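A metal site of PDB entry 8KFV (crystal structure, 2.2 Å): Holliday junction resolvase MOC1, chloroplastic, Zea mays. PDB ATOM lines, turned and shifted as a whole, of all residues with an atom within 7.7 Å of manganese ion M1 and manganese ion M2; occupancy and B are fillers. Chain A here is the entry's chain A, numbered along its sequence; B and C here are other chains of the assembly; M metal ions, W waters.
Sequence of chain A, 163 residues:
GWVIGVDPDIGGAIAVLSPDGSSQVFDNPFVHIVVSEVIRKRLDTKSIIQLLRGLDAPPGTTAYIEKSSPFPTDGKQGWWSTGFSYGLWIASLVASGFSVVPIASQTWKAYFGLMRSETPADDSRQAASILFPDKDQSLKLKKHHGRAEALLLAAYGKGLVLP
OP1 of DC 25 of chain C lies within salt-bridge range of the side-chain amino group (NZ) of Lys 109 (2.5 Å). The backbone NH (N) of Glu 66 is in hydrogen-bond range of the backbone carbonyl oxygen (O) of Val 6. The side-chain carboxylate (OD1) of Asp 9 lies within hydrogen-bond range of the backbone NH (N) of Gly 11 (3.0 Å). The backbone NH (N) of Asp 7 lies within hydrogen-bond range of the backbone carbonyl oxygen (O) of Ala 13 (2.9 Å). The backbone carbonyl oxygen (O) of Asp 7 is in hydrogen-bond range of the side-chain amide nitrogen (ND2) of Asn 28, 2.9 Å away. OP3 of DC 1 of chain B lies close to O3' of DC 25 of chain C. OE2 of Glu 66 sits at hydrogen-bond distance from NE1 of Trp 108, at 3.0 Å. The side-chain carboxylate of Asp 9 is in hydrogen-bond range of the backbone NH of Gly 12 (3.0 Å).
Four residues have an atom within 4 Å of manganese ion M1: Asp 7, Asp 9, Glu 149 and DC 1 of chain B.
Of the 23 residues printed, 6 come within 4 Å of manganese ion M2.
Manganese ion M1 is bound by the side-chain carboxylate (OD2) of Asp 7 (2.1 Å). OE1 of Glu 149 binds manganese ion M1 (2.2 Å). Water W3 is bound to manganese ion M1. Manganese ion M1 is bound by OD2 of Asp 9. Manganese ion M1 is bound by OP3 of DC 1 of chain B, 2.3 Å away. Manganese ion M1 has five donor atoms within binding distance. Slightly farther from manganese ion M1 lies OP2 of DC 1 of chain B (2.7 Å).
Manganese ion M2 is bound by the side-chain carboxylate (OE1) of Glu 66 (2.1 Å), the side-chain carboxylate (OD1) of Asp 7 (2.2 Å), water W1 (2.2 Å), OP3 of DC 1 of chain B (2.2 Å) and water W2 (2.3 Å). Manganese ion M2 has five donor atoms within binding distance. Slightly farther from manganese ion M2 lies O3' of DC 25 of chain C (2.8 Å).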
ATOM      1  N   VAL A   6      -6.550 -29.172 -11.631  1.00  0.00           N
ATOM      2  CA  VAL A   6      -8.004 -29.030 -11.451  1.00  0.00           C
ATOM      3  C   VAL A   6      -8.324 -27.707 -10.767  1.00  0.00           C
ATOM      4  O   VAL A   6      -7.876 -27.453  -9.646  1.00  0.00           O
ATOM      5  CB  VAL A   6      -8.618 -30.187 -10.641  1.00  0.00           C
ATOM      6  CG1 VAL A   6     -10.143 -29.912 -10.422  1.00  0.00           C
ATOM      7  CG2 VAL A   6      -8.425 -31.524 -11.333  1.00  0.00           C
ATOM      8  N   ASP A   7      -9.107 -26.881 -11.456  1.00  0.00           N
ATOM      9  CA  ASP A   7      -9.814 -25.766 -10.857  1.00  0.00           C
ATOM     10  C   ASP A   7     -11.222 -26.254 -10.528  1.00  0.00           C
ATOM     11  O   ASP A   7     -12.019 -26.465 -11.461  1.00  0.00           O
ATOM     12  CB  ASP A   7      -9.848 -24.593 -11.837  1.00  0.00           C
ATOM     13  CG  ASP A   7     -10.433 -23.322 -11.233  1.00  0.00           C
ATOM     14  OD1 ASP A   7     -10.091 -22.986 -10.085  1.00  0.00           O
ATOM     15  OD2 ASP A   7     -11.205 -22.631 -11.930  1.00  0.00           O
ATOM     16  N   PRO A   8     -11.564 -26.494  -9.263  1.00  0.00           N
ATOM     17  CA  PRO A   8     -12.755 -27.299  -8.945  1.00  0.00           C
ATOM     18  C   PRO A   8     -14.093 -26.566  -8.965  1.00  0.00           C
ATOM     19  O   PRO A   8     -15.118 -27.222  -8.730  1.00  0.00           O
ATOM     20  CB  PRO A   8     -12.456 -27.805  -7.516  1.00  0.00           C
ATOM     21  CG  PRO A   8     -11.642 -26.685  -6.916  1.00  0.00           C
ATOM     22  CD  PRO A   8     -10.793 -26.144  -8.062  1.00  0.00           C
ATOM     23  N   ASP A   9     -14.164 -25.260  -9.227  1.00  0.00           N
ATOM     24  CA  ASP A   9     -15.437 -24.564  -9.079  1.00  0.00           C
ATOM     25  C   ASP A   9     -16.367 -24.849 -10.275  1.00  0.00           C
ATOM     26  O   ASP A   9     -16.029 -25.600 -11.203  1.00  0.00           O
ATOM     27  CB  ASP A   9     -15.219 -23.056  -8.856  1.00  0.00           C
ATOM     28  CG  ASP A   9     -14.516 -22.337 -10.044  1.00  0.00           C
ATOM     29  OD1 ASP A   9     -15.168 -22.130 -11.104  1.00  0.00           O
ATOM     30  OD2 ASP A   9     -13.329 -21.919  -9.890  1.00  0.00           O
ATOM     31  N   ILE A  10     -17.560 -24.256 -10.237  1.00  0.00           N
ATOM     32  CA  ILE A  10     -18.614 -24.620 -11.195  1.00  0.00           C
ATOM     33  C   ILE A  10     -18.268 -24.131 -12.603  1.00  0.00           C
ATOM     34  O   ILE A  10     -18.720 -24.720 -13.597  1.00  0.00           O
ATOM     35  CB  ILE A  10     -19.981 -24.076 -10.726  1.00  0.00           C
ATOM     36  CG1 ILE A  10     -21.110 -24.987 -11.180  1.00  0.00           C
ATOM     37  CG2 ILE A  10     -20.222 -22.676 -11.255  1.00  0.00           C
ATOM     38  CD1 ILE A  10     -21.019 -26.391 -10.647  1.00  0.00           C
ATOM     39  N   GLY A  11     -17.463 -23.086 -12.724  1.00  0.00           N
ATOM     40  CA  GLY A  11     -16.943 -22.684 -14.025  1.00  0.00           C
ATOM     41  C   GLY A  11     -15.483 -23.071 -14.191  1.00  0.00           C
ATOM     42  O   GLY A  11     -14.754 -22.471 -14.981  1.00  0.00           O
ATOM     43  N   GLY A  12     -15.054 -24.077 -13.448  1.00  0.00           N
ATOM     44  CA  GLY A  12     -13.685 -24.544 -13.502  1.00  0.00           C
ATOM     45  C   GLY A  12     -13.446 -25.507 -14.641  1.00  0.00           C
ATOM     46  O   GLY A  12     -14.265 -25.635 -15.563  1.00  0.00           O
ATOM     47  N   ALA A  13     -12.324 -26.200 -14.562  1.00  0.00           N
ATOM     48  CA  ALA A  13     -11.873 -27.069 -15.639  1.00  0.00           C
ATOM     49  C   ALA A  13     -10.805 -28.005 -15.099  1.00  0.00           C
ATOM     50  O   ALA A  13     -10.247 -27.792 -14.012  1.00  0.00           O
ATOM     51  CB  ALA A  13     -11.307 -26.261 -16.831  1.00  0.00           C
ATOM     52  N   ASN A  28     -15.496 -28.160 -16.535  1.00  0.00           N
ATOM     53  CA  ASN A  28     -16.129 -29.009 -15.522  1.00  0.00           C
ATOM     54  C   ASN A  28     -17.558 -29.343 -15.945  1.00  0.00           C
ATOM     55  O   ASN A  28     -18.323 -28.425 -16.278  1.00  0.00           O
ATOM     56  CB  ASN A  28     -16.103 -28.328 -14.154  1.00  0.00           C
ATOM     57  CG  ASN A  28     -14.726 -28.350 -13.552  1.00  0.00           C
ATOM     58  OD1 ASN A  28     -13.840 -29.007 -14.099  1.00  0.00           O
ATOM     59  ND2 ASN A  28     -14.532 -27.669 -12.427  1.00  0.00           N
ATOM     60  N   GLU A  66      -6.658 -26.659  -6.710  1.00  0.00           N
ATOM     61  CA  GLU A  66      -6.669 -25.450  -5.898  1.00  0.00           C
ATOM     62  C   GLU A  66      -7.378 -25.699  -4.554  1.00  0.00           C
ATOM     63  O   GLU A  66      -8.516 -26.191  -4.528  1.00  0.00           O
ATOM     64  CB  GLU A  66      -7.356 -24.340  -6.677  1.00  0.00           C
ATOM     65  CG  GLU A  66      -7.025 -22.961  -6.160  1.00  0.00           C
ATOM     66  CD  GLU A  66      -7.642 -21.891  -7.017  1.00  0.00           C
ATOM     67  OE1 GLU A  66      -8.890 -21.766  -6.963  1.00  0.00           O
ATOM     68  OE2 GLU A  66      -6.886 -21.205  -7.755  1.00  0.00           O
ATOM     69  N   LYS A  67      -6.700 -25.398  -3.447  1.00  0.00           N
ATOM     70  CA  LYS A  67      -7.292 -25.569  -2.131  1.00  0.00           C
ATOM     71  C   LYS A  67      -8.507 -24.679  -1.998  1.00  0.00           C
ATOM     72  O   LYS A  67      -8.501 -23.537  -2.475  1.00  0.00           O
ATOM     73  CB  LYS A  67      -6.326 -25.194  -1.011  1.00  0.00           C
ATOM     74  CG  LYS A  67      -5.116 -26.058  -0.833  1.00  0.00           C
ATOM     75  CD  LYS A  67      -4.315 -25.634   0.402  1.00  0.00           C
ATOM     76  CE  LYS A  67      -2.988 -26.359   0.442  1.00  0.00           C
ATOM     77  NZ  LYS A  67      -2.248 -26.052   1.679  1.00  0.00           N
ATOM     78  N   SER A 105      -4.067 -20.839  -4.005  1.00  0.00           N
ATOM     79  CA  SER A 105      -4.046 -19.937  -5.149  1.00  0.00           C
ATOM     80  C   SER A 105      -2.894 -18.960  -5.053  1.00  0.00           C
ATOM     81  O   SER A 105      -2.351 -18.534  -6.087  1.00  0.00           O
ATOM     82  CB  SER A 105      -5.367 -19.178  -5.267  1.00  0.00           C
ATOM     83  OG  SER A 105      -5.475 -18.246  -4.211  1.00  0.00           O
ATOM     84  N   TRP A 108       0.444 -20.704  -6.785  1.00  0.00           N
ATOM     85  CA  TRP A 108       0.686 -20.736  -8.219  1.00  0.00           C
ATOM     86  C   TRP A 108       0.661 -19.331  -8.820  1.00  0.00           C
ATOM     87  O   TRP A 108       1.356 -19.077  -9.823  1.00  0.00           O
ATOM     88  CB  TRP A 108      -0.285 -21.684  -8.939  1.00  0.00           C
ATOM     89  CG  TRP A 108      -1.741 -21.303  -8.973  1.00  0.00           C
ATOM     90  CD1 TRP A 108      -2.723 -21.784  -8.157  1.00  0.00           C
ATOM     91  CD2 TRP A 108      -2.375 -20.393  -9.873  1.00  0.00           C
ATOM     92  NE1 TRP A 108      -3.928 -21.227  -8.486  1.00  0.00           N
ATOM     93  CE2 TRP A 108      -3.754 -20.372  -9.543  1.00  0.00           C
ATOM     94  CE3 TRP A 108      -1.928 -19.591 -10.934  1.00  0.00           C
ATOM     95  CZ2 TRP A 108      -4.675 -19.583 -10.225  1.00  0.00           C
ATOM     96  CZ3 TRP A 108      -2.839 -18.818 -11.603  1.00  0.00           C
ATOM     97  CH2 TRP A 108      -4.201 -18.809 -11.262  1.00  0.00           C
ATOM     98  N   LYS A 109      -0.087 -18.408  -8.224  1.00  0.00           N
ATOM     99  CA  LYS A 109      -0.029 -17.017  -8.689  1.00  0.00           C
ATOM    100  C   LYS A 109       1.353 -16.414  -8.474  1.00  0.00           C
ATOM    101  O   LYS A 109       1.926 -15.835  -9.403  1.00  0.00           O
ATOM    102  CB  LYS A 109      -1.101 -16.176  -8.005  1.00  0.00           C
ATOM    103  CG  LYS A 109      -2.507 -16.458  -8.550  1.00  0.00           C
ATOM    104  CD  LYS A 109      -3.517 -15.417  -8.121  1.00  0.00           C
ATOM    105  CE  LYS A 109      -4.922 -15.807  -8.600  1.00  0.00           C
ATOM    106  NZ  LYS A 109      -5.616 -14.669  -9.284  1.00  0.00           N
ATOM    107  N   HIS A 145     -11.566 -18.208 -18.018  1.00  0.00           N
ATOM    108  CA  HIS A 145     -10.492 -18.122 -17.043  1.00  0.00           C
ATOM    109  C   HIS A 145     -10.361 -19.404 -16.216  1.00  0.00           C
ATOM    110  O   HIS A 145      -9.280 -19.662 -15.685  1.00  0.00           O
ATOM    111  CB  HIS A 145     -10.669 -16.893 -16.129  1.00  0.00           C
ATOM    112  CG  HIS A 145     -11.874 -16.946 -15.249  1.00  0.00           C
ATOM    113  ND1 HIS A 145     -11.838 -17.485 -13.974  1.00  0.00           N
ATOM    114  CD2 HIS A 145     -13.138 -16.505 -15.426  1.00  0.00           C
ATOM    115  CE1 HIS A 145     -13.037 -17.389 -13.419  1.00  0.00           C
ATOM    116  NE2 HIS A 145     -13.844 -16.784 -14.281  1.00  0.00           N
ATOM    117  N   GLY A 146     -11.424 -20.198 -16.098  1.00  0.00           N
ATOM    118  CA  GLY A 146     -11.307 -21.472 -15.401  1.00  0.00           C
ATOM    119  C   GLY A 146     -10.417 -22.448 -16.139  1.00  0.00           C
ATOM    120  O   GLY A 146      -9.583 -23.139 -15.533  1.00  0.00           O
ATOM    121  N   ARG A 147     -10.580 -22.544 -17.460  1.00  0.00           N
ATOM    122  CA  ARG A 147      -9.631 -23.275 -18.282  1.00  0.00           C
ATOM    123  C   ARG A 147      -8.206 -22.796 -18.057  1.00  0.00           C
ATOM    124  O   ARG A 147      -7.287 -23.595 -17.886  1.00  0.00           O
ATOM    125  CB  ARG A 147     -10.009 -23.145 -19.748  1.00  0.00           C
ATOM    126  CG  ARG A 147     -11.385 -23.638 -20.112  1.00  0.00           C
ATOM    127  CD  ARG A 147     -11.669 -23.343 -21.583  1.00  0.00           C
ATOM    128  NE  ARG A 147     -13.007 -23.761 -21.994  1.00  0.00           N
ATOM    129  CZ  ARG A 147     -13.451 -23.679 -23.242  1.00  0.00           C
ATOM    130  NH1 ARG A 147     -12.699 -23.152 -24.210  1.00  0.00           N
ATOM    131  NH2 ARG A 147     -14.653 -24.143 -23.537  1.00  0.00           N
ATOM    132  N   GLU A 149      -6.961 -21.280 -15.392  1.00  0.00           N
ATOM    133  CA  GLU A 149      -6.529 -21.636 -14.046  1.00  0.00           C
ATOM    134  C   GLU A 149      -6.091 -23.108 -13.975  1.00  0.00           C
ATOM    135  O   GLU A 149      -5.042 -23.429 -13.393  1.00  0.00           O
ATOM    136  CB  GLU A 149      -7.660 -21.348 -13.050  1.00  0.00           C
ATOM    137  CG  GLU A 149      -7.720 -19.890 -12.580  1.00  0.00           C
ATOM    138  CD  GLU A 149      -9.137 -19.357 -12.249  1.00  0.00           C
ATOM    139  OE1 GLU A 149     -10.135 -20.124 -12.268  1.00  0.00           O
ATOM    140  OE2 GLU A 149      -9.249 -18.145 -11.986  1.00  0.00           O
ATOM    141  N   ALA A 150      -6.878 -24.004 -14.576  1.00  0.00           N
ATOM    142  CA  ALA A 150      -6.536 -25.419 -14.619  1.00  0.00           C
ATOM    143  C   ALA A 150      -5.203 -25.635 -15.331  1.00  0.00           C
ATOM    144  O   ALA A 150      -4.367 -26.411 -14.867  1.00  0.00           O
ATOM    145  CB  ALA A 150      -7.644 -26.216 -15.327  1.00  0.00           C
ATOM    146  N   LEU A 153      -2.366 -24.342 -13.150  1.00  0.00           N
ATOM    147  CA  LEU A 153      -2.089 -25.261 -12.037  1.00  0.00           C
ATOM    148  C   LEU A 153      -1.246 -26.421 -12.520  1.00  0.00           C
ATOM    149  O   LEU A 153      -0.258 -26.808 -11.877  1.00  0.00           O
ATOM    150  CB  LEU A 153      -3.391 -25.784 -11.416  1.00  0.00           C
ATOM    151  CG  LEU A 153      -4.039 -24.963 -10.325  1.00  0.00           C
ATOM    152  CD1 LEU A 153      -5.510 -25.303 -10.275  1.00  0.00           C
ATOM    153  CD2 LEU A 153      -3.386 -25.252  -8.991  1.00  0.00           C
ATOM    154  OP3  DC B   1     -11.349 -19.686  -9.300  1.00  0.00           O
ATOM    155  P    DC B   1     -12.302 -18.572  -9.076  1.00  0.00           P
ATOM    156  OP1  DC B   1     -11.612 -17.336  -8.668  1.00  0.00           O
ATOM    157  OP2  DC B   1     -13.192 -18.506 -10.278  1.00  0.00           O
ATOM    158  O5'  DC B   1     -13.199 -19.019  -7.848  1.00  0.00           O
ATOM    159  C5'  DC B   1     -14.592 -19.225  -8.053  1.00  0.00           C
ATOM    160  C4'  DC B   1     -15.305 -19.478  -6.744  1.00  0.00           C
ATOM    161  O4'  DC B   1     -14.962 -18.434  -5.795  1.00  0.00           O
ATOM    162  C3'  DC B   1     -16.802 -19.450  -6.854  1.00  0.00           C
ATOM    163  O3'  DC B   1     -17.262 -20.737  -7.122  1.00  0.00           O
ATOM    164  C2'  DC B   1     -17.256 -18.981  -5.471  1.00  0.00           C
ATOM    165  C1'  DC B   1     -16.089 -18.123  -4.986  1.00  0.00           C
ATOM    166  N1   DC B   1     -16.342 -16.639  -5.035  1.00  0.00           N
ATOM    167  C2   DC B   1     -17.390 -16.086  -4.271  1.00  0.00           C
ATOM    168  O2   DC B   1     -18.088 -16.824  -3.577  1.00  0.00           O
ATOM    169  N3   DC B   1     -17.590 -14.750  -4.302  1.00  0.00           N
ATOM    170  C4   DC B   1     -16.804 -13.955  -5.047  1.00  0.00           C
ATOM    171  N4   DC B   1     -17.049 -12.649  -5.029  1.00  0.00           N
ATOM    172  C5   DC B   1     -15.734 -14.488  -5.833  1.00  0.00           C
ATOM    173  C6   DC B   1     -15.531 -15.829  -5.793  1.00  0.00           C
ATOM    174  P    DA B   2     -18.658 -20.972  -7.892  1.00  0.00           P
ATOM    175  OP1  DA B   2     -18.739 -22.445  -8.055  1.00  0.00           O
ATOM    176  OP2  DA B   2     -18.731 -20.069  -9.071  1.00  0.00           O
ATOM    177  O5'  DA B   2     -19.791 -20.479  -6.860  1.00  0.00           O
ATOM    178  C5'  DA B   2     -19.933 -21.120  -5.592  1.00  0.00           C
ATOM    179  C4'  DA B   2     -21.186 -20.625  -4.886  1.00  0.00           C
ATOM    180  O4'  DA B   2     -21.080 -19.221  -4.544  1.00  0.00           O
ATOM    181  C3'  DA B   2     -22.476 -20.758  -5.692  1.00  0.00           C
ATOM    182  O3'  DA B   2     -23.534 -21.059  -4.814  1.00  0.00           O
ATOM    183  C2'  DA B   2     -22.653 -19.361  -6.302  1.00  0.00           C
ATOM    184  C1'  DA B   2     -22.083 -18.466  -5.212  1.00  0.00           C
ATOM    185  N9   DA B   2     -21.427 -17.269  -5.730  1.00  0.00           N
ATOM    186  C8   DA B   2     -20.399 -17.249  -6.633  1.00  0.00           C
ATOM    187  N7   DA B   2     -19.966 -16.050  -6.900  1.00  0.00           N
ATOM    188  C5   DA B   2     -20.747 -15.214  -6.125  1.00  0.00           C
ATOM    189  C6   DA B   2     -20.777 -13.824  -5.984  1.00  0.00           C
ATOM    190  N6   DA B   2     -19.939 -13.020  -6.651  1.00  0.00           N
ATOM    191  N1   DA B   2     -21.683 -13.289  -5.127  1.00  0.00           N
ATOM    192  C2   DA B   2     -22.508 -14.131  -4.470  1.00  0.00           C
ATOM    193  N3   DA B   2     -22.575 -15.471  -4.544  1.00  0.00           N
ATOM    194  C4   DA B   2     -21.662 -15.945  -5.398  1.00  0.00           C
ATOM    195  P    DC C  25      -8.105 -14.654  -6.556  1.00  0.00           P
ATOM    196  OP1  DC C  25      -7.753 -14.844  -7.984  1.00  0.00           O
ATOM    197  OP2  DC C  25      -8.692 -13.367  -6.129  1.00  0.00           O
ATOM    198  O5'  DC C  25      -9.126 -15.819  -6.114  1.00  0.00           O
ATOM    199  C5'  DC C  25      -8.620 -17.160  -5.962  1.00  0.00           C
ATOM    200  C4'  DC C  25      -9.582 -18.019  -5.184  1.00  0.00           C
ATOM    201  O4'  DC C  25     -10.026 -17.311  -4.009  1.00  0.00           O
ATOM    202  C3'  DC C  25     -10.862 -18.358  -5.914  1.00  0.00           C
ATOM    203  O3'  DC C  25     -10.668 -19.466  -6.757  1.00  0.00           O
ATOM    204  C2'  DC C  25     -11.806 -18.700  -4.772  1.00  0.00           C
ATOM    205  C1'  DC C  25     -11.333 -17.748  -3.669  1.00  0.00           C
ATOM    206  N1   DC C  25     -12.215 -16.551  -3.466  1.00  0.00           N
ATOM    207  C2   DC C  25     -13.374 -16.710  -2.708  1.00  0.00           C
ATOM    208  O2   DC C  25     -13.638 -17.818  -2.251  1.00  0.00           O
ATOM    209  N3   DC C  25     -14.162 -15.629  -2.499  1.00  0.00           N
ATOM    210  C4   DC C  25     -13.842 -14.444  -3.021  1.00  0.00           C
ATOM    211  N4   DC C  25     -14.677 -13.426  -2.789  1.00  0.00           N
ATOM    212  C5   DC C  25     -12.663 -14.269  -3.814  1.00  0.00           C
ATOM    213  C6   DC C  25     -11.877 -15.338  -4.005  1.00  0.00           C
HETATM  214 MN    MN M   1     -11.950 -20.763 -11.186  1.00  0.00          MN
HETATM  215 MN    MN M   2     -10.039 -21.333  -8.692  1.00  0.00          MN
HETATM  216  O   HOH W   1      -8.750 -19.663  -9.218  1.00  0.00           O
HETATM  217  O   HOH W   2     -11.883 -22.411  -7.970  1.00  0.00           O
HETATM  218  O   HOH W   3     -13.527 -20.624 -12.725  1.00  0.00           O
